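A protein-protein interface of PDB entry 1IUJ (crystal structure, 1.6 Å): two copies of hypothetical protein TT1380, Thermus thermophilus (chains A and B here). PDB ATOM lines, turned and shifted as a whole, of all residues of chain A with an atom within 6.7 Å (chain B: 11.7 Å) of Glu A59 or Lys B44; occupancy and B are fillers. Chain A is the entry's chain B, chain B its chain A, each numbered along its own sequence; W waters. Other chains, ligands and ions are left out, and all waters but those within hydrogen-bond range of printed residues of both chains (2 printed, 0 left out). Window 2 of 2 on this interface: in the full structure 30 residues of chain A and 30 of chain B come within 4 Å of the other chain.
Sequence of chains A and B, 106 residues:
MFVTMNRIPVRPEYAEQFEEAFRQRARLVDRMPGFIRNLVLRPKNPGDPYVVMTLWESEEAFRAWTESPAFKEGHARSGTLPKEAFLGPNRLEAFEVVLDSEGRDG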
ATOM      1  N   MET A   1     -14.201 -34.782  10.882  1.00  0.00           N
ATOM      2  CA  MET A   1     -15.324 -34.480   9.942  1.00  0.00           C
ATOM      3  C   MET A   1     -14.809 -33.748   8.710  1.00  0.00           C
ATOM      4  O   MET A   1     -13.973 -32.843   8.814  1.00  0.00           O
ATOM      5  CB  MET A   1     -16.437 -33.698  10.658  1.00  0.00           C
ATOM      6  CG  MET A   1     -17.749 -33.758   9.937  1.00  0.00           C
ATOM      7  SD  MET A   1     -19.179 -33.010  10.770  1.00  0.00           S
ATOM      8  CE  MET A   1     -18.732 -31.379  10.652  1.00  0.00           C
ATOM      9  N   PHE A   2     -15.281 -34.160   7.544  1.00  0.00           N
ATOM     10  CA  PHE A   2     -14.779 -33.682   6.261  1.00  0.00           C
ATOM     11  C   PHE A   2     -15.940 -32.958   5.577  1.00  0.00           C
ATOM     12  O   PHE A   2     -17.076 -33.421   5.641  1.00  0.00           O
ATOM     13  CB  PHE A   2     -14.284 -34.880   5.444  1.00  0.00           C
ATOM     14  CG  PHE A   2     -13.919 -34.570   4.015  1.00  0.00           C
ATOM     15  CD1 PHE A   2     -12.642 -34.096   3.693  1.00  0.00           C
ATOM     16  CD2 PHE A   2     -14.818 -34.826   2.991  1.00  0.00           C
ATOM     17  CE1 PHE A   2     -12.276 -33.833   2.361  1.00  0.00           C
ATOM     18  CE2 PHE A   2     -14.476 -34.576   1.618  1.00  0.00           C
ATOM     19  CZ  PHE A   2     -13.192 -34.081   1.311  1.00  0.00           C
ATOM     20  N   VAL A   3     -15.683 -31.791   4.999  1.00  0.00           N
ATOM     21  CA  VAL A   3     -16.754 -31.003   4.399  1.00  0.00           C
ATOM     22  C   VAL A   3     -16.409 -30.656   2.964  1.00  0.00           C
ATOM     23  O   VAL A   3     -15.267 -30.227   2.673  1.00  0.00           O
ATOM     24  CB  VAL A   3     -16.973 -29.678   5.198  1.00  0.00           C
ATOM     25  CG1 VAL A   3     -17.974 -28.773   4.527  1.00  0.00           C
ATOM     26  CG2 VAL A   3     -17.378 -29.975   6.624  1.00  0.00           C
ATOM     27  N   TRP A  56     -19.308 -35.002   6.018  1.00  0.00           N
ATOM     28  CA  TRP A  56     -18.986 -36.444   5.957  1.00  0.00           C
ATOM     29  C   TRP A  56     -18.149 -36.863   7.160  1.00  0.00           C
ATOM     30  O   TRP A  56     -17.375 -36.073   7.699  1.00  0.00           O
ATOM     31  CB  TRP A  56     -18.135 -36.681   4.690  1.00  0.00           C
ATOM     32  CG  TRP A  56     -18.910 -36.511   3.383  1.00  0.00           C
ATOM     33  CD1 TRP A  56     -18.876 -35.451   2.517  1.00  0.00           C
ATOM     34  CD2 TRP A  56     -19.760 -37.489   2.787  1.00  0.00           C
ATOM     35  NE1 TRP A  56     -19.707 -35.688   1.444  1.00  0.00           N
ATOM     36  CE2 TRP A  56     -20.247 -36.944   1.577  1.00  0.00           C
ATOM     37  CE3 TRP A  56     -20.167 -38.779   3.157  1.00  0.00           C
ATOM     38  CZ2 TRP A  56     -21.142 -37.639   0.749  1.00  0.00           C
ATOM     39  CZ3 TRP A  56     -21.058 -39.467   2.329  1.00  0.00           C
ATOM     40  CH2 TRP A  56     -21.516 -38.902   1.143  1.00  0.00           C
ATOM     41  N   GLU A  57     -18.261 -38.135   7.573  1.00  0.00           N
ATOM     42  CA  GLU A  57     -17.418 -38.640   8.660  1.00  0.00           C
ATOM     43  C   GLU A  57     -15.923 -38.575   8.333  1.00  0.00           C
ATOM     44  O   GLU A  57     -15.088 -38.397   9.228  1.00  0.00           O
ATOM     45  CB  GLU A  57     -17.810 -40.101   8.952  1.00  0.00           C
ATOM     46  CG  GLU A  57     -17.192 -40.728  10.169  1.00  0.00           C
ATOM     47  CD  GLU A  57     -18.140 -40.634  11.339  1.00  0.00           C
ATOM     48  OE1 GLU A  57     -18.156 -39.559  11.975  1.00  0.00           O
ATOM     49  OE2 GLU A  57     -18.893 -41.620  11.594  1.00  0.00           O
ATOM     50  N   SER A  58     -15.596 -38.713   7.040  1.00  0.00           N
ATOM     51  CA  SER A  58     -14.219 -38.714   6.570  1.00  0.00           C
ATOM     52  C   SER A  58     -14.135 -38.422   5.102  1.00  0.00           C
ATOM     53  O   SER A  58     -15.111 -38.573   4.384  1.00  0.00           O
ATOM     54  CB  SER A  58     -13.552 -40.069   6.825  1.00  0.00           C
ATOM     55  OG  SER A  58     -14.109 -41.092   5.986  1.00  0.00           O
ATOM     56  N   GLU A  59     -12.938 -38.054   4.645  1.00  0.00           N
ATOM     57  CA  GLU A  59     -12.692 -37.925   3.223  1.00  0.00           C
ATOM     58  C   GLU A  59     -12.963 -39.247   2.463  1.00  0.00           C
ATOM     59  O   GLU A  59     -13.504 -39.228   1.358  1.00  0.00           O
ATOM     60  CB  GLU A  59     -11.278 -37.392   2.997  1.00  0.00           C
ATOM     61  CG  GLU A  59     -10.930 -37.201   1.527  1.00  0.00           C
ATOM     62  CD  GLU A  59      -9.549 -36.605   1.318  1.00  0.00           C
ATOM     63  OE1 GLU A  59      -8.825 -36.273   2.288  1.00  0.00           O
ATOM     64  OE2 GLU A  59      -9.185 -36.512   0.154  1.00  0.00           O
ATOM     65  N   GLU A  60     -12.578 -40.367   3.069  1.00  0.00           N
ATOM     66  CA  GLU A  60     -12.794 -41.674   2.454  1.00  0.00           C
ATOM     67  C   GLU A  60     -14.284 -41.913   2.183  1.00  0.00           C
ATOM     68  O   GLU A  60     -14.652 -42.454   1.146  1.00  0.00           O
ATOM     69  CB  GLU A  60     -12.166 -42.768   3.317  1.00  0.00           C
ATOM     70  CG  GLU A  60     -12.232 -44.184   2.708  1.00  0.00           C
ATOM     71  CD  GLU A  60     -11.500 -44.314   1.379  1.00  0.00           C
ATOM     72  OE1 GLU A  60     -10.687 -43.445   1.021  1.00  0.00           O
ATOM     73  OE2 GLU A  60     -11.707 -45.331   0.671  1.00  0.00           O
ATOM     74  N   ALA A  61     -15.131 -41.547   3.143  1.00  0.00           N
ATOM     75  CA  ALA A  61     -16.576 -41.679   2.944  1.00  0.00           C
ATOM     76  C   ALA A  61     -17.061 -40.863   1.736  1.00  0.00           C
ATOM     77  O   ALA A  61     -17.861 -41.356   0.932  1.00  0.00           O
ATOM     78  CB  ALA A  61     -17.333 -41.307   4.229  1.00  0.00           C
ATOM     79  N   PHE A  62     -16.575 -39.619   1.605  1.00  0.00           N
ATOM     80  CA  PHE A  62     -16.777 -38.852   0.404  1.00  0.00           C
ATOM     81  C   PHE A  62     -16.288 -39.565  -0.859  1.00  0.00           C
ATOM     82  O   PHE A  62     -17.034 -39.642  -1.853  1.00  0.00           O
ATOM     83  CB  PHE A  62     -16.121 -37.480   0.564  1.00  0.00           C
ATOM     84  CG  PHE A  62     -16.017 -36.737  -0.697  1.00  0.00           C
ATOM     85  CD1 PHE A  62     -14.790 -36.670  -1.381  1.00  0.00           C
ATOM     86  CD2 PHE A  62     -17.139 -36.085  -1.210  1.00  0.00           C
ATOM     87  CE1 PHE A  62     -14.665 -35.992  -2.545  1.00  0.00           C
ATOM     88  CE2 PHE A  62     -17.038 -35.385  -2.393  1.00  0.00           C
ATOM     89  CZ  PHE A  62     -15.757 -35.315  -3.068  1.00  0.00           C
ATOM     90  N   ARG A  63     -15.072 -40.110  -0.839  1.00  0.00           N
ATOM     91  CA  ARG A  63     -14.561 -40.777  -2.046  1.00  0.00           C
ATOM     92  C   ARG A  63     -15.448 -41.963  -2.448  1.00  0.00           C
ATOM     93  O   ARG A  63     -15.755 -42.127  -3.601  1.00  0.00           O
ATOM     94  CB  ARG A  63     -13.141 -41.276  -1.889  1.00  0.00           C
ATOM     95  CG  ARG A  63     -12.105 -40.178  -1.491  1.00  0.00           C
ATOM     96  CD  ARG A  63     -11.075 -40.642  -0.385  1.00  0.00           C
ATOM     97  NE  ARG A  63      -9.733 -40.014  -0.391  1.00  0.00           N
ATOM     98  CZ  ARG A  63      -8.837 -40.055   0.599  1.00  0.00           C
ATOM     99  NH1 ARG A  63      -9.079 -40.674   1.749  1.00  0.00           N
ATOM    100  NH2 ARG A  63      -7.662 -39.431   0.453  1.00  0.00           N
ATOM    101  N   ALA A  64     -15.881 -42.760  -1.484  1.00  0.00           N
ATOM    102  CA  ALA A  64     -16.758 -43.896  -1.793  1.00  0.00           C
ATOM    103  C   ALA A  64     -18.059 -43.413  -2.441  1.00  0.00           C
ATOM    104  O   ALA A  64     -18.573 -43.972  -3.427  1.00  0.00           O
ATOM    105  CB  ALA A  64     -17.024 -44.675  -0.539  1.00  0.00           C
ATOM    106  N   GLU A  93     -14.713 -27.080  -3.327  1.00  0.00           N
ATOM    107  CA  GLU A  93     -13.764 -26.855  -2.240  1.00  0.00           C
ATOM    108  C   GLU A  93     -13.957 -27.968  -1.196  1.00  0.00           C
ATOM    109  O   GLU A  93     -15.074 -28.483  -1.039  1.00  0.00           O
ATOM    110  CB  GLU A  93     -14.069 -25.527  -1.577  1.00  0.00           C
ATOM    111  CG  GLU A  93     -13.849 -24.315  -2.461  1.00  0.00           C
ATOM    112  CD  GLU A  93     -13.772 -23.045  -1.639  1.00  0.00           C
ATOM    113  OE1 GLU A  93     -12.693 -22.431  -1.665  1.00  0.00           O
ATOM    114  OE2 GLU A  93     -14.777 -22.706  -1.008  1.00  0.00           O
ATOM    115  N   ALA A  94     -12.900 -28.340  -0.477  1.00  0.00           N
ATOM    116  CA  ALA A  94     -12.989 -29.381   0.533  1.00  0.00           C
ATOM    117  C   ALA A  94     -12.194 -28.978   1.749  1.00  0.00           C
ATOM    118  O   ALA A  94     -11.198 -28.240   1.611  1.00  0.00           O
ATOM    119  CB  ALA A  94     -12.428 -30.683  -0.013  1.00  0.00           C
ATOM    120  N   PHE A  95     -12.638 -29.459   2.913  1.00  0.00           N
ATOM    121  CA  PHE A  95     -12.094 -28.998   4.214  1.00  0.00           C
ATOM    122  C   PHE A  95     -12.121 -30.099   5.253  1.00  0.00           C
ATOM    123  O   PHE A  95     -12.939 -31.042   5.195  1.00  0.00           O
ATOM    124  CB  PHE A  95     -12.921 -27.832   4.818  1.00  0.00           C
ATOM    125  CG  PHE A  95     -13.167 -26.671   3.877  1.00  0.00           C
ATOM    126  CD1 PHE A  95     -14.208 -26.716   2.944  1.00  0.00           C
ATOM    127  CD2 PHE A  95     -12.381 -25.524   3.937  1.00  0.00           C
ATOM    128  CE1 PHE A  95     -14.438 -25.656   2.081  1.00  0.00           C
ATOM    129  CE2 PHE A  95     -12.616 -24.442   3.077  1.00  0.00           C
ATOM    130  CZ  PHE A  95     -13.637 -24.516   2.139  1.00  0.00           C
ATOM    131  N   GLU A  96     -11.270 -29.926   6.268  1.00  0.00           N
ATOM    132  CA  GLU A  96     -11.341 -30.687   7.506  1.00  0.00           C
ATOM    133  C   GLU A  96     -11.839 -29.750   8.561  1.00  0.00           C
ATOM    134  O   GLU A  96     -11.367 -28.598   8.647  1.00  0.00           O
ATOM    135  CB  GLU A  96      -9.958 -31.220   7.864  1.00  0.00           C
ATOM    136  CG  GLU A  96      -9.551 -32.403   6.993  1.00  0.00           C
ATOM    137  CD  GLU A  96     -10.334 -33.673   7.259  1.00  0.00           C
ATOM    138  OE1 GLU A  96     -10.849 -33.875   8.388  1.00  0.00           O
ATOM    139  OE2 GLU A  96     -10.419 -34.487   6.301  1.00  0.00           O
ATOM    140  N   ARG B   7     -14.334 -16.099   4.537  1.00  0.00           N
ATOM    141  CA  ARG B   7     -13.211 -16.751   3.872  1.00  0.00           C
ATOM    142  C   ARG B   7     -11.937 -16.028   4.204  1.00  0.00           C
ATOM    143  O   ARG B   7     -11.774 -14.859   3.890  1.00  0.00           O
ATOM    144  CB  ARG B   7     -13.429 -16.792   2.360  1.00  0.00           C
ATOM    145  CG  ARG B   7     -14.743 -17.461   1.970  1.00  0.00           C
ATOM    146  CD  ARG B   7     -15.125 -17.294   0.502  1.00  0.00           C
ATOM    147  NE  ARG B   7     -14.084 -17.860  -0.328  1.00  0.00           N
ATOM    148  CZ  ARG B   7     -13.991 -19.182  -0.573  1.00  0.00           C
ATOM    149  NH1 ARG B   7     -14.894 -20.008  -0.059  1.00  0.00           N
ATOM    150  NH2 ARG B   7     -12.995 -19.643  -1.309  1.00  0.00           N
ATOM    151  N   ILE B   8     -11.051 -16.721   4.914  1.00  0.00           N
ATOM    152  CA  ILE B   8      -9.854 -16.110   5.491  1.00  0.00           C
ATOM    153  C   ILE B   8      -8.592 -16.649   4.782  1.00  0.00           C
ATOM    154  O   ILE B   8      -8.195 -17.783   5.001  1.00  0.00           O
ATOM    155  CB  ILE B   8      -9.807 -16.423   6.993  1.00  0.00           C
ATOM    156  CG1 ILE B   8     -11.138 -16.063   7.685  1.00  0.00           C
ATOM    157  CG2 ILE B   8      -8.638 -15.672   7.664  1.00  0.00           C
ATOM    158  CD1 ILE B   8     -11.585 -17.143   8.510  1.00  0.00           C
ATOM    159  N   VAL B  10      -5.438 -16.921   5.021  1.00  0.00           N
ATOM    160  CA  VAL B  10      -4.239 -17.005   5.860  1.00  0.00           C
ATOM    161  C   VAL B  10      -3.158 -17.828   5.173  1.00  0.00           C
ATOM    162  O   VAL B  10      -3.425 -18.852   4.545  1.00  0.00           O
ATOM    163  CB  VAL B  10      -4.577 -17.483   7.284  1.00  0.00           C
ATOM    164  CG1 VAL B  10      -5.100 -18.843   7.298  1.00  0.00           C
ATOM    165  CG2 VAL B  10      -3.407 -17.336   8.243  1.00  0.00           C
ATOM    166  N   PRO B  12      -0.052 -20.431   5.006  1.00  0.00           N
ATOM    167  CA  PRO B  12       0.097 -21.689   5.770  1.00  0.00           C
ATOM    168  C   PRO B  12       0.997 -21.535   7.013  1.00  0.00           C
ATOM    169  O   PRO B  12       0.668 -22.120   8.062  1.00  0.00           O
ATOM    170  CB  PRO B  12       0.681 -22.679   4.736  1.00  0.00           C
ATOM    171  CG  PRO B  12       1.119 -21.862   3.599  1.00  0.00           C
ATOM    172  CD  PRO B  12       0.303 -20.608   3.582  1.00  0.00           C
ATOM    173  N   ALA B  15      -1.131 -20.485   9.789  1.00  0.00           N
ATOM    174  CA  ALA B  15      -2.422 -21.139   9.987  1.00  0.00           C
ATOM    175  C   ALA B  15      -2.615 -21.631  11.427  1.00  0.00           C
ATOM    176  O   ALA B  15      -3.699 -21.482  11.962  1.00  0.00           O
ATOM    177  CB  ALA B  15      -2.661 -22.279   8.969  1.00  0.00           C
ATOM    178  N   GLU B  19      -5.684 -20.551  13.898  1.00  0.00           N
ATOM    179  CA  GLU B  19      -6.588 -21.532  14.463  1.00  0.00           C
ATOM    180  C   GLU B  19      -6.626 -21.360  15.967  1.00  0.00           C
ATOM    181  O   GLU B  19      -7.697 -21.323  16.566  1.00  0.00           O
ATOM    182  CB  GLU B  19      -6.125 -22.969  14.175  1.00  0.00           C
ATOM    183  CG  GLU B  19      -6.306 -23.436  12.739  1.00  0.00           C
ATOM    184  CD  GLU B  19      -5.907 -24.885  12.512  1.00  0.00           C
ATOM    185  OE1 GLU B  19      -5.727 -25.630  13.494  1.00  0.00           O
ATOM    186  OE2 GLU B  19      -5.760 -25.303  11.355  1.00  0.00           O
ATOM    187  N   VAL B  40     -15.033 -24.011  12.200  1.00  0.00           N
ATOM    188  CA  VAL B  40     -13.851 -23.463  11.533  1.00  0.00           C
ATOM    189  C   VAL B  40     -13.361 -24.582  10.622  1.00  0.00           C
ATOM    190  O   VAL B  40     -13.133 -25.681  11.108  1.00  0.00           O
ATOM    191  CB  VAL B  40     -12.744 -23.061  12.508  1.00  0.00           C
ATOM    192  CG1 VAL B  40     -11.537 -22.487  11.765  1.00  0.00           C
ATOM    193  CG2 VAL B  40     -13.263 -22.026  13.563  1.00  0.00           C
ATOM    194  N   LEU B  41     -13.232 -24.310   9.313  1.00  0.00           N
ATOM    195  CA  LEU B  41     -12.881 -25.338   8.303  1.00  0.00           C
ATOM    196  C   LEU B  41     -11.499 -25.022   7.700  1.00  0.00           C
ATOM    197  O   LEU B  41     -11.252 -23.918   7.176  1.00  0.00           O
ATOM    198  CB  LEU B  41     -13.907 -25.294   7.174  1.00  0.00           C
ATOM    199  CG  LEU B  41     -15.343 -25.411   7.638  1.00  0.00           C
ATOM    200  CD1 LEU B  41     -16.288 -25.202   6.472  1.00  0.00           C
ATOM    201  CD2 LEU B  41     -15.582 -26.741   8.330  1.00  0.00           C
ATOM    202  N   ARG B  42     -10.590 -25.994   7.782  1.00  0.00           N
ATOM    203  CA  ARG B  42      -9.253 -25.844   7.231  1.00  0.00           C
ATOM    204  C   ARG B  42      -9.293 -26.443   5.812  1.00  0.00           C
ATOM    205  O   ARG B  42      -9.733 -27.589   5.625  1.00  0.00           O
ATOM    206  CB  ARG B  42      -8.240 -26.614   8.062  1.00  0.00           C
ATOM    207  CG  ARG B  42      -6.871 -26.702   7.420  1.00  0.00           C
ATOM    208  CD  ARG B  42      -5.857 -27.575   8.158  1.00  0.00           C
ATOM    209  NE  ARG B  42      -6.363 -28.887   8.547  1.00  0.00           N
ATOM    210  CZ  ARG B  42      -6.440 -29.268   9.841  1.00  0.00           C
ATOM    211  NH1 ARG B  42      -6.032 -28.435  10.799  1.00  0.00           N
ATOM    212  NH2 ARG B  42      -6.911 -30.462  10.183  1.00  0.00           N
ATOM    213  N   PRO B  43      -8.759 -25.723   4.825  1.00  0.00           N
ATOM    214  CA  PRO B  43      -8.773 -26.231   3.455  1.00  0.00           C
ATOM    215  C   PRO B  43      -7.885 -27.432   3.281  1.00  0.00           C
ATOM    216  O   PRO B  43      -6.851 -27.555   3.946  1.00  0.00           O
ATOM    217  CB  PRO B  43      -8.225 -25.045   2.642  1.00  0.00           C
ATOM    218  CG  PRO B  43      -7.291 -24.352   3.620  1.00  0.00           C
ATOM    219  CD  PRO B  43      -8.064 -24.421   4.915  1.00  0.00           C
ATOM    220  N   LYS B  44      -8.272 -28.311   2.362  1.00  0.00           N
ATOM    221  CA  LYS B  44      -7.345 -29.415   2.062  1.00  0.00           C
ATOM    222  C   LYS B  44      -6.050 -28.960   1.397  1.00  0.00           C
ATOM    223  O   LYS B  44      -4.989 -29.527   1.696  1.00  0.00           O
ATOM    224  CB  LYS B  44      -8.002 -30.486   1.205  1.00  0.00           C
ATOM    225  CG  LYS B  44      -9.158 -31.176   1.886  1.00  0.00           C
ATOM    226  CD  LYS B  44      -8.758 -31.998   3.105  1.00  0.00           C
ATOM    227  CE  LYS B  44      -7.888 -33.170   2.728  1.00  0.00           C
ATOM    228  NZ  LYS B  44      -8.182 -34.304   3.700  1.00  0.00           N
ATOM    229  N   ASN B  45      -6.131 -27.940   0.563  1.00  0.00           N
ATOM    230  CA  ASN B  45      -4.955 -27.318  -0.028  1.00  0.00           C
ATOM    231  C   ASN B  45      -4.551 -26.116   0.831  1.00  0.00           C
ATOM    232  O   ASN B  45      -5.304 -25.141   0.951  1.00  0.00           O
ATOM    233  CB  ASN B  45      -5.262 -26.851  -1.431  1.00  0.00           C
ATOM    234  CG  ASN B  45      -4.118 -26.106  -2.022  1.00  0.00           C
ATOM    235  OD1 ASN B  45      -2.990 -26.224  -1.557  1.00  0.00           O
ATOM    236  ND2 ASN B  45      -4.396 -25.291  -2.988  1.00  0.00           N
ATOM    237  N   PRO B  46      -3.366 -26.170   1.438  1.00  0.00           N
ATOM    238  CA  PRO B  46      -2.892 -25.054   2.280  1.00  0.00           C
ATOM    239  C   PRO B  46      -2.785 -23.706   1.541  1.00  0.00           C
ATOM    240  O   PRO B  46      -2.736 -22.661   2.196  1.00  0.00           O
ATOM    241  CB  PRO B  46      -1.515 -25.526   2.770  1.00  0.00           C
ATOM    242  CG  PRO B  46      -1.157 -26.638   1.921  1.00  0.00           C
ATOM    243  CD  PRO B  46      -2.426 -27.305   1.432  1.00  0.00           C
ATOM    244  N   GLY B  47      -2.799 -23.717   0.211  1.00  0.00           N
ATOM    245  CA  GLY B  47      -2.917 -22.495  -0.589  1.00  0.00           C
ATOM    246  C   GLY B  47      -4.305 -21.834  -0.720  1.00  0.00           C
ATOM    247  O   GLY B  47      -4.421 -20.730  -1.294  1.00  0.00           O
ATOM    248  N   ASP B  48      -5.333 -22.485  -0.152  1.00  0.00           N
ATOM    249  CA  ASP B  48      -6.702 -21.962  -0.189  1.00  0.00           C
ATOM    250  C   ASP B  48      -7.106 -21.363   1.163  1.00  0.00           C
ATOM    251  O   ASP B  48      -6.428 -21.579   2.158  1.00  0.00           O
ATOM    252  CB  ASP B  48      -7.690 -23.082  -0.529  1.00  0.00           C
ATOM    253  CG  ASP B  48      -7.570 -23.565  -1.952  1.00  0.00           C
ATOM    254  OD1 ASP B  48      -7.194 -22.764  -2.830  1.00  0.00           O
ATOM    255  OD2 ASP B  48      -7.836 -24.733  -2.260  1.00  0.00           O
ATOM    256  N   PRO B  49      -8.178 -20.566   1.208  1.00  0.00           N
ATOM    257  CA  PRO B  49      -8.568 -19.934   2.470  1.00  0.00           C
ATOM    258  C   PRO B  49      -9.298 -20.882   3.418  1.00  0.00           C
ATOM    259  O   PRO B  49      -9.957 -21.829   3.003  1.00  0.00           O
ATOM    260  CB  PRO B  49      -9.528 -18.823   2.045  1.00  0.00           C
ATOM    261  CG  PRO B  49     -10.071 -19.254   0.730  1.00  0.00           C
ATOM    262  CD  PRO B  49      -9.064 -20.166   0.088  1.00  0.00           C
ATOM    263  N   TYR B  50      -9.127 -20.619   4.707  1.00  0.00           N
ATOM    264  CA  TYR B  50      -9.997 -21.139   5.738  1.00  0.00           C
ATOM    265  C   TYR B  50     -11.404 -20.589   5.558  1.00  0.00           C
ATOM    266  O   TYR B  50     -11.595 -19.538   4.976  1.00  0.00           O
ATOM    267  CB  TYR B  50      -9.474 -20.680   7.103  1.00  0.00           C
ATOM    268  CG  TYR B  50      -8.411 -21.577   7.697  1.00  0.00           C
ATOM    269  CD1 TYR B  50      -7.139 -21.603   7.160  1.00  0.00           C
ATOM    270  CD2 TYR B  50      -8.694 -22.417   8.773  1.00  0.00           C
ATOM    271  CE1 TYR B  50      -6.139 -22.413   7.698  1.00  0.00           C
ATOM    272  CE2 TYR B  50      -7.682 -23.253   9.325  1.00  0.00           C
ATOM    273  CZ  TYR B  50      -6.420 -23.230   8.757  1.00  0.00           C
ATOM    274  OH  TYR B  50      -5.408 -24.012   9.232  1.00  0.00           O
ATOM    275  N   VAL B  51     -12.400 -21.323   6.043  1.00  0.00           N
ATOM    276  CA  VAL B  51     -13.742 -20.782   6.109  1.00  0.00           C
ATOM    277  C   VAL B  51     -14.241 -20.836   7.550  1.00  0.00           C
ATOM    278  O   VAL B  51     -14.196 -21.897   8.158  1.00  0.00           O
ATOM    279  CB  VAL B  51     -14.703 -21.519   5.199  1.00  0.00           C
ATOM    280  CG1 VAL B  51     -16.120 -21.060   5.494  1.00  0.00           C
ATOM    281  CG2 VAL B  51     -14.340 -21.286   3.723  1.00  0.00           C
HETATM  282  O   HOH W   1     -10.896 -22.974   0.564  1.00  0.00           O
HETATM  283  O   HOH W   2     -17.472 -22.282  -0.702  1.00  0.00           O
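CA of Pro B43 touches O of Ala A94, at 3.6 Å. Phe A95 touches Leu B41. CA of Phe A95 touches O of Arg B42, 3.1 Å away. CD2 of Phe A95 touches CA of Pro B43, at 3.7 Å. Phe A95 touches Pro B49 (CE2 to O, 3.7 Å). Val B51 touches Phe A95. O of Glu A96 touches CA of Leu B41, 3.6 Å away.
Water W2 lies within hydrogen-bond range of the side-chain carboxylate (OE2) of Glu A93 (2.7 Å) and the guanidinium group (NH1) of Arg B7 (3.5 Å). Water W1 bridges the backbone carbonyl oxygen of Pro B49 (2.9 Å) and the side-chain carboxylate of Glu A93 (2.9 Å).
No position is printed for both chains.
Hydrophobic or aromatic side chains of chain B that line the printed part of chain A: Leu B41 and Val B51. Hydrophobic or aromatic side chains of chain A that line the printed part of chain B: Ala A94 and Phe A95. Among the printed residues, 12 pairs touch across the chains. Among the printed residues, Asp or Glu carboxylates within 4 Å of a Lys or Arg side-chain nitrogen of the other chain: Glu A59 with Lys B44 (2.5 Å), Glu A93 with Arg B7 (2.8 Å) and Glu A96 with Lys B44 (3.4 Å).
No residue of chain B comes within 4 Å of Phe A2. Glu A57 touches none of the printed residues of chain B. No residue of chain B comes within 4 Å of Ser A58. Glu A59 touches just one residue of chain B: Lys B44. No residue of chain B comes within 4 Å of Glu A60. No residue of chain B comes within 4 Å of Ala A61. Phe A62 touches none of the printed residues of chain B. Ala A94 touches just these residues of chain B: Pro B43 (3.6 Å) and Lys B44 (3.0 Å). Glu A96 touches just these residues of chain B: Leu B41, Arg B42 and Lys B44. Of the printed residues of chain A, Leu B41 touches Phe A95 (3.6 Å) and Glu A96 (3.6 Å). Of the printed residues of chain A, Arg B42 touches Phe A95 and Glu A96. Of the printed residues of chain A, Pro B43 touches Ala A94 and Phe A95. Of the printed residues of chain A, Lys B44 touches Glu A59 (2.5 Å), Ala A94 (3.0 Å) and Glu A96 (3.4 Å). The nearest printed residue of chain B that does not touch Glu A59 is Asn B45 (8.9 Å). The nearest printed residue of chain A that does not touch Lys B44 is Phe A95 (4.01 Å).
The guanidinium group (NH1) of Arg B42 lies within salt-bridge range of the side-chain carboxylate (OE2) of Glu B19, 3.2 Å away. The backbone NH of Leu B41 is in hydrogen-bond range of the backbone carbonyl oxygen of Val B51 (2.8 Å). The backbone carbonyl oxygen (O) of Val A3 sits at hydrogen-bond distance from the backbone NH (N) of Phe A95 (2.7 Å). OE2 of Glu A59 is in salt-bridge range of NH2 of Arg A63 (3.3 Å).
NH2 of Arg B7 is in salt-bridge range of OE1 of Glu A93 (2.8 Å). O of Glu A96 sits at hydrogen-bond distance from N of Arg B42. The side-chain carboxylate (OE1) of Glu A59 is in salt-bridge range of the side-chain amino group (NZ) of Lys B44, at 2.5 Å. The backbone NH of Lys B44 is in hydrogen-bond range of the backbone carbonyl oxygen of Ala A94, at 3.0 Å. NZ of Lys B44 lies within salt-bridge range of OE2 of Glu A96.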
